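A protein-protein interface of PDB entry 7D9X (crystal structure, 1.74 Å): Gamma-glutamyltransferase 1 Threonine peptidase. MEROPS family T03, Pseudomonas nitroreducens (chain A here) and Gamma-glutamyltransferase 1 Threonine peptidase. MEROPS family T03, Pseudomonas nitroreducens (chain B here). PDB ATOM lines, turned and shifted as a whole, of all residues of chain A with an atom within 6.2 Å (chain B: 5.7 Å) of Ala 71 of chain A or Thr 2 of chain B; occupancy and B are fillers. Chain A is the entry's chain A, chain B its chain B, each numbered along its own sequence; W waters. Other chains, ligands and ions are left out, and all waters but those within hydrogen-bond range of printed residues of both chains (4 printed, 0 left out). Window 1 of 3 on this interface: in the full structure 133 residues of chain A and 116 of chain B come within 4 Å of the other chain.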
ATOM      1  N   PRO A  35      19.227   1.285  -3.526  1.00  0.00           N
ATOM      2  CA  PRO A  35      19.597   1.084  -2.117  1.00  0.00           C
ATOM      3  C   PRO A  35      18.532   0.410  -1.270  1.00  0.00           C
ATOM      4  O   PRO A  35      18.809   0.112  -0.103  1.00  0.00           O
ATOM      5  CB  PRO A  35      19.853   2.517  -1.624  1.00  0.00           C
ATOM      6  CG  PRO A  35      18.884   3.344  -2.447  1.00  0.00           C
ATOM      7  CD  PRO A  35      18.960   2.703  -3.838  1.00  0.00           C
ATOM      8  N   LEU A  64      12.220   6.545  -3.167  1.00  0.00           N
ATOM      9  CA  LEU A  64      13.125   6.547  -2.017  1.00  0.00           C
ATOM     10  C   LEU A  64      12.885   7.746  -1.118  1.00  0.00           C
ATOM     11  O   LEU A  64      13.209   7.687   0.077  1.00  0.00           O
ATOM     12  CB  LEU A  64      14.572   6.481  -2.490  1.00  0.00           C
ATOM     13  CG  LEU A  64      14.952   5.235  -3.286  1.00  0.00           C
ATOM     14  CD1 LEU A  64      16.307   5.428  -3.955  1.00  0.00           C
ATOM     15  CD2 LEU A  64      14.930   3.971  -2.432  1.00  0.00           C
ATOM     16  N   TYR A  68      13.046   5.639   1.991  1.00  0.00           N
ATOM     17  CA  TYR A  68      14.426   5.789   2.471  1.00  0.00           C
ATOM     18  C   TYR A  68      14.631   7.200   3.022  1.00  0.00           C
ATOM     19  O   TYR A  68      15.570   7.904   2.654  1.00  0.00           O
ATOM     20  CB  TYR A  68      15.398   5.480   1.335  1.00  0.00           C
ATOM     21  CG  TYR A  68      16.711   4.827   1.694  1.00  0.00           C
ATOM     22  CD1 TYR A  68      17.792   5.594   2.091  1.00  0.00           C
ATOM     23  CD2 TYR A  68      16.876   3.439   1.621  1.00  0.00           C
ATOM     24  CE1 TYR A  68      19.005   5.006   2.419  1.00  0.00           C
ATOM     25  CE2 TYR A  68      18.091   2.843   1.949  1.00  0.00           C
ATOM     26  CZ  TYR A  68      19.151   3.634   2.347  1.00  0.00           C
ATOM     27  OH  TYR A  68      20.363   3.046   2.670  1.00  0.00           O
ATOM     28  N   PRO A  69      13.771   7.636   3.942  1.00  0.00           N
ATOM     29  CA  PRO A  69      13.775   9.059   4.346  1.00  0.00           C
ATOM     30  C   PRO A  69      15.049   9.513   5.023  1.00  0.00           C
ATOM     31  O   PRO A  69      15.297  10.726   5.110  1.00  0.00           O
ATOM     32  CB  PRO A  69      12.581   9.157   5.317  1.00  0.00           C
ATOM     33  CG  PRO A  69      12.447   7.785   5.876  1.00  0.00           C
ATOM     34  CD  PRO A  69      12.792   6.839   4.693  1.00  0.00           C
ATOM     35  N   GLU A  70      15.882   8.585   5.487  1.00  0.00           N
ATOM     36  CA  GLU A  70      17.159   9.017   6.044  1.00  0.00           C
ATOM     37  C   GLU A  70      18.035   9.704   5.003  1.00  0.00           C
ATOM     38  O   GLU A  70      18.885  10.513   5.366  1.00  0.00           O
ATOM     39  CB  GLU A  70      17.866   7.820   6.673  1.00  0.00           C
ATOM     40  CG  GLU A  70      18.166   6.667   5.722  1.00  0.00           C
ATOM     41  CD  GLU A  70      17.088   5.596   5.718  1.00  0.00           C
ATOM     42  OE1 GLU A  70      15.870   5.918   5.733  1.00  0.00           O
ATOM     43  OE2 GLU A  70      17.477   4.395   5.725  1.00  0.00           O
ATOM     44  N   ALA A  71      17.814   9.443   3.707  1.00  0.00           N
ATOM     45  CA  ALA A  71      18.621  10.073   2.668  1.00  0.00           C
ATOM     46  C   ALA A  71      17.821  10.395   1.410  1.00  0.00           C
ATOM     47  O   ALA A  71      17.967  11.486   0.842  1.00  0.00           O
ATOM     48  CB  ALA A  71      19.809   9.174   2.277  1.00  0.00           C
ATOM     49  N   GLY A  72      17.025   9.440   0.934  1.00  0.00           N
ATOM     50  CA  GLY A  72      16.089   9.751  -0.135  1.00  0.00           C
ATOM     51  C   GLY A  72      15.166  10.869   0.309  1.00  0.00           C
ATOM     52  O   GLY A  72      14.797  10.953   1.483  1.00  0.00           O
ATOM     53  N   ASN A  73      14.801  11.744  -0.631  1.00  0.00           N
ATOM     54  CA  ASN A  73      14.285  13.027  -0.177  1.00  0.00           C
ATOM     55  C   ASN A  73      13.605  13.799  -1.290  1.00  0.00           C
ATOM     56  O   ASN A  73      13.930  13.643  -2.470  1.00  0.00           O
ATOM     57  CB  ASN A  73      15.436  13.893   0.382  1.00  0.00           C
ATOM     58  CG  ASN A  73      16.397  14.372  -0.725  1.00  0.00           C
ATOM     59  OD1 ASN A  73      16.188  15.417  -1.365  1.00  0.00           O
ATOM     60  ND2 ASN A  73      17.468  13.615  -0.948  1.00  0.00           N
ATOM     61  N   THR B   1      22.958  10.190   2.863  1.00  0.00           N
ATOM     62  CA  THR B   1      23.132  10.140   1.402  1.00  0.00           C
ATOM     63  C   THR B   1      22.745   8.778   0.877  1.00  0.00           C
ATOM     64  O   THR B   1      22.812   7.793   1.599  1.00  0.00           O
ATOM     65  CB  THR B   1      24.589  10.455   1.035  1.00  0.00           C
ATOM     66  OG1 THR B   1      24.949  11.733   1.589  1.00  0.00           O
ATOM     67  CG2 THR B   1      24.825  10.459  -0.461  1.00  0.00           C
ATOM     68  N   THR B   2      22.307   8.710  -0.385  1.00  0.00           N
ATOM     69  CA  THR B   2      22.094   7.410  -1.022  1.00  0.00           C
ATOM     70  C   THR B   2      22.337   7.562  -2.516  1.00  0.00           C
ATOM     71  O   THR B   2      22.335   8.675  -3.050  1.00  0.00           O
ATOM     72  CB  THR B   2      20.691   6.845  -0.723  1.00  0.00           C
ATOM     73  OG1 THR B   2      20.656   5.446  -1.074  1.00  0.00           O
ATOM     74  CG2 THR B   2      19.610   7.597  -1.475  1.00  0.00           C
ATOM     75  N   HIS B   3      22.591   6.427  -3.175  1.00  0.00           N
ATOM     76  CA  HIS B   3      22.893   6.397  -4.598  1.00  0.00           C
ATOM     77  C   HIS B   3      22.117   5.280  -5.283  1.00  0.00           C
ATOM     78  O   HIS B   3      21.975   4.185  -4.724  1.00  0.00           O
ATOM     79  CB  HIS B   3      24.391   6.160  -4.862  1.00  0.00           C
ATOM     80  CG  HIS B   3      24.748   6.189  -6.313  1.00  0.00           C
ATOM     81  ND1 HIS B   3      25.041   7.358  -6.975  1.00  0.00           N
ATOM     82  CD2 HIS B   3      24.837   5.195  -7.235  1.00  0.00           C
ATOM     83  CE1 HIS B   3      25.292   7.091  -8.244  1.00  0.00           C
ATOM     84  NE2 HIS B   3      25.180   5.784  -8.428  1.00  0.00           N
ATOM     85  N   PHE B   4      21.684   5.522  -6.521  1.00  0.00           N
ATOM     86  CA  PHE B   4      21.189   4.438  -7.360  1.00  0.00           C
ATOM     87  C   PHE B   4      21.705   4.603  -8.781  1.00  0.00           C
ATOM     88  O   PHE B   4      22.051   5.706  -9.222  1.00  0.00           O
ATOM     89  CB  PHE B   4      19.660   4.345  -7.331  1.00  0.00           C
ATOM     90  CG  PHE B   4      18.950   5.588  -7.788  1.00  0.00           C
ATOM     91  CD1 PHE B   4      18.679   5.788  -9.145  1.00  0.00           C
ATOM     92  CD2 PHE B   4      18.520   6.532  -6.875  1.00  0.00           C
ATOM     93  CE1 PHE B   4      18.004   6.922  -9.558  1.00  0.00           C
ATOM     94  CE2 PHE B   4      17.858   7.664  -7.289  1.00  0.00           C
ATOM     95  CZ  PHE B   4      17.589   7.862  -8.632  1.00  0.00           C
ATOM     96  N   ASN B  16      22.804   8.488 -10.012  1.00  0.00           N
ATOM     97  CA  ASN B  16      22.182   9.561  -9.240  1.00  0.00           C
ATOM     98  C   ASN B  16      22.500   9.425  -7.762  1.00  0.00           C
ATOM     99  O   ASN B  16      22.088   8.459  -7.115  1.00  0.00           O
ATOM    100  CB  ASN B  16      20.665   9.575  -9.446  1.00  0.00           C
ATOM    101  CG  ASN B  16      20.018  10.779  -8.816  1.00  0.00           C
ATOM    102  OD1 ASN B  16      19.914  11.834  -9.446  1.00  0.00           O
ATOM    103  ND2 ASN B  16      19.603  10.640  -7.564  1.00  0.00           N
ATOM    104  N   THR B  17      23.216  10.405  -7.219  1.00  0.00           N
ATOM    105  CA  THR B  17      23.452  10.497  -5.784  1.00  0.00           C
ATOM    106  C   THR B  17      22.689  11.710  -5.269  1.00  0.00           C
ATOM    107  O   THR B  17      22.776  12.782  -5.861  1.00  0.00           O
ATOM    108  CB  THR B  17      24.936  10.657  -5.469  1.00  0.00           C
ATOM    109  OG1 THR B  17      25.725   9.762  -6.273  1.00  0.00           O
ATOM    110  CG2 THR B  17      25.201  10.380  -3.984  1.00  0.00           C
ATOM    111  N   TYR B  18      21.935  11.535  -4.191  1.00  0.00           N
ATOM    112  CA  TYR B  18      21.239  12.660  -3.583  1.00  0.00           C
ATOM    113  C   TYR B  18      21.110  12.387  -2.087  1.00  0.00           C
ATOM    114  O   TYR B  18      21.426  11.292  -1.592  1.00  0.00           O
ATOM    115  CB  TYR B  18      19.897  12.944  -4.297  1.00  0.00           C
ATOM    116  CG  TYR B  18      18.727  12.010  -4.067  1.00  0.00           C
ATOM    117  CD1 TYR B  18      18.907  10.668  -3.814  1.00  0.00           C
ATOM    118  CD2 TYR B  18      17.421  12.494  -4.140  1.00  0.00           C
ATOM    119  CE1 TYR B  18      17.814   9.828  -3.612  1.00  0.00           C
ATOM    120  CE2 TYR B  18      16.323  11.669  -3.945  1.00  0.00           C
ATOM    121  CZ  TYR B  18      16.531  10.337  -3.673  1.00  0.00           C
ATOM    122  OH  TYR B  18      15.447   9.518  -3.475  1.00  0.00           O
ATOM    123  N   THR B  19      20.675  13.408  -1.350  1.00  0.00           N
ATOM    124  CA  THR B  19      20.919  13.364   0.092  1.00  0.00           C
ATOM    125  C   THR B  19      20.208  14.482   0.835  1.00  0.00           C
ATOM    126  O   THR B  19      19.824  15.500   0.260  1.00  0.00           O
ATOM    127  CB  THR B  19      22.436  13.457   0.388  1.00  0.00           C
ATOM    128  OG1 THR B  19      22.669  13.256   1.784  1.00  0.00           O
ATOM    129  CG2 THR B  19      22.989  14.826  -0.045  1.00  0.00           C
ATOM    130  N   LEU B  20      20.105  14.283   2.150  1.00  0.00           N
ATOM    131  CA  LEU B  20      19.782  15.317   3.122  1.00  0.00           C
ATOM    132  C   LEU B  20      21.031  15.805   3.845  1.00  0.00           C
ATOM    133  O   LEU B  20      20.926  16.708   4.685  1.00  0.00           O
ATOM    134  CB  LEU B  20      18.789  14.773   4.149  1.00  0.00           C
ATOM    135  CG  LEU B  20      17.360  14.501   3.669  1.00  0.00           C
ATOM    136  CD1 LEU B  20      16.564  13.774   4.726  1.00  0.00           C
ATOM    137  CD2 LEU B  20      16.666  15.801   3.248  1.00  0.00           C
ATOM    138  N   PHE B  24      18.454  11.713   8.071  1.00  0.00           N
ATOM    139  CA  PHE B  24      17.256  12.509   8.323  1.00  0.00           C
ATOM    140  C   PHE B  24      17.555  14.007   8.397  1.00  0.00           C
ATOM    141  O   PHE B  24      16.728  14.790   8.908  1.00  0.00           O
ATOM    142  CB  PHE B  24      16.555  12.053   9.611  1.00  0.00           C
ATOM    143  CG  PHE B  24      16.268  10.583   9.662  1.00  0.00           C
ATOM    144  CD1 PHE B  24      15.110  10.062   9.066  1.00  0.00           C
ATOM    145  CD2 PHE B  24      17.129   9.719  10.311  1.00  0.00           C
ATOM    146  CE1 PHE B  24      14.841   8.712   9.128  1.00  0.00           C
ATOM    147  CE2 PHE B  24      16.863   8.362  10.364  1.00  0.00           C
ATOM    148  CZ  PHE B  24      15.731   7.856   9.772  1.00  0.00           C
ATOM    149  N   THR B  91      27.993   6.082  -4.614  1.00  0.00           N
ATOM    150  CA  THR B  91      27.878   5.646  -3.223  1.00  0.00           C
ATOM    151  C   THR B  91      27.644   6.856  -2.325  1.00  0.00           C
ATOM    152  O   THR B  91      28.063   7.969  -2.658  1.00  0.00           O
ATOM    153  CB  THR B  91      29.154   4.910  -2.761  1.00  0.00           C
ATOM    154  OG1 THR B  91      29.022   4.554  -1.392  1.00  0.00           O
ATOM    155  CG2 THR B  91      30.364   5.811  -2.944  1.00  0.00           C
ATOM    156  N   PRO B  92      27.033   6.657  -1.161  1.00  0.00           N
ATOM    157  CA  PRO B  92      27.119   7.647  -0.081  1.00  0.00           C
ATOM    158  C   PRO B  92      28.461   7.523   0.633  1.00  0.00           C
ATOM    159  O   PRO B  92      29.286   6.677   0.306  1.00  0.00           O
ATOM    160  CB  PRO B  92      25.962   7.256   0.837  1.00  0.00           C
ATOM    161  CG  PRO B  92      25.851   5.762   0.657  1.00  0.00           C
ATOM    162  CD  PRO B  92      26.136   5.540  -0.810  1.00  0.00           C
ATOM    163  N   ASP B 166      27.950   2.554   0.265  1.00  0.00           N
ATOM    164  CA  ASP B 166      26.841   1.684  -0.121  1.00  0.00           C
ATOM    165  C   ASP B 166      26.824   1.732  -1.643  1.00  0.00           C
ATOM    166  O   ASP B 166      25.953   2.391  -2.235  1.00  0.00           O
ATOM    167  CB  ASP B 166      25.531   2.133   0.503  1.00  0.00           C
ATOM    168  CG  ASP B 166      24.424   1.095   0.341  1.00  0.00           C
ATOM    169  OD1 ASP B 166      24.672   0.004  -0.216  1.00  0.00           O
ATOM    170  OD2 ASP B 166      23.290   1.352   0.808  1.00  0.00           O
HETATM  171  O   HOH W   1      22.330   4.131   0.775  1.00  0.00           O
HETATM  172  O   HOH W   2      21.031  11.892   4.058  1.00  0.00           O
HETATM  173  O   HOH W   3      23.613   2.352   3.545  1.00  0.00           O
HETATM  174  O   HOH W   4      20.850   0.508   1.487  1.00  0.00           O
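O of Glu 70 of chain A sits at hydrogen-bond distance from N of Phe 24 of chain B, 3.0 Å away.
ND2 of Asn 73 of chain A sits close to N of Thr 19 of chain B (3.2 Å).
The side-chain amide nitrogen (ND2) of Asn 73 of chain A is in hydrogen-bond range of the backbone carbonyl oxygen (O) of Ala 71 of chain A, at 2.8 Å.
The side-chain hydroxyl (OG1) of Thr 1 of chain B sits at hydrogen-bond distance from the side-chain hydroxyl (OG1) of Thr 19 of chain B (2.7 Å).
The backbone carbonyl oxygen (O) of Tyr 18 of chain B lies within hydrogen-bond range of the backbone NH (N) of Thr 2 of chain B, 3.0 Å away.
A ring nitrogen (ND1) of His 3 of chain B sits at hydrogen-bond distance from the backbone carbonyl oxygen (O) of Asn 16 of chain B.
The side-chain hydroxyl (OG1) of Thr 17 of chain B sits at hydrogen-bond distance from a ring nitrogen (ND1) of His 3 of chain B (2.6 Å).
The backbone carbonyl oxygen (O) of Phe 4 of chain B lies within hydrogen-bond range of the backbone NH (N) of Asn 16 of chain B (3.0 Å).
Pro 35 of chain A touches Thr 2 of chain B.
Pro 35 of chain A touches His 3 of chain B.
Phe 4 of chain B touches Leu 64 of chain A.
OG1 of Thr 2 of chain B touches CE1 of Tyr 68 of chain A (3.9 Å).
Asp 166 of chain B touches Tyr 68 of chain A (OD2 to OH, 3.9 Å).
O of Pro 69 of chain A touches CD1 of Leu 20 of chain B (3.3 Å).
Ala 71 of chain A touches Leu 20 of chain B (O to N, 3.8 Å).
Gly 72 of chain A touches Tyr 18 of chain B.
Asn 73 of chain A touches Tyr 18 of chain B (ND2 to CD2, 3.4 Å).
Leu 20 of chain B touches Asn 73 of chain A.
Of the printed residues of chain A, Thr 2 of chain B touches Pro 35, Tyr 68, Ala 71 and Gly 72.
Of the printed residues of chain A, Phe 24 of chain B touches Glu 70.
Printed residues of chain B within 4 Å of Pro 35 of chain A: Thr 2 (3.1 Å), His 3 (3.5 Å) and Phe 4 (3.9 Å).
Printed residues of chain B within 4 Å of Leu 64 of chain A: Phe 4 (3.8 Å) and Tyr 18 (3.3 Å).
Printed residues of chain A within 4 Å of Asp 166 of chain B: Tyr 68.
Of the printed residues of chain A, Leu 20 of chain B touches Pro 69, Ala 71 and Asn 73.
Pro 92 of chain B touches none of the printed residues of chain A.
The nearest printed residue of chain B that does not touch Ala 71 of chain A is Tyr 18 of chain B (4.2 Å).
The nearest printed residue of chain A that does not touch Thr 2 of chain B is Leu 64 of chain A (4.7 Å).
The nearest printed residue of chain B that does not touch Glu 70 of chain A is Leu 20 of chain B (4.1 Å).
Of the 13 printed residues of chain B, 9 touch a printed residue of chain A.
Water W4 lies within hydrogen-bond range of O of Pro 35 of chain A (2.6 Å), OD2 of Asp 166 of chain B (2.7 Å) and OH of Tyr 68 of chain A (2.8 Å).
Water W1 lies within hydrogen-bond range of OG1 of Thr 2 of chain B, OH of Tyr 68 of chain A and OD2 of Asp 166 of chain B.
Water W2 lies within hydrogen-bond range of the backbone NH (N) of Thr 1 of chain B (2.8 Å), the backbone carbonyl oxygen (O) of Glu 70 of chain A (2.9 Å), the side-chain hydroxyl (OG1) of Thr 19 of chain B (3.1 Å) and the backbone NH (N) of Leu 20 of chain B (3.2 Å).
Water W3 lies within hydrogen-bond range of OD2 of Asp 166 of chain B (2.9 Å) and OH of Tyr 68 of chain A (3.4 Å).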
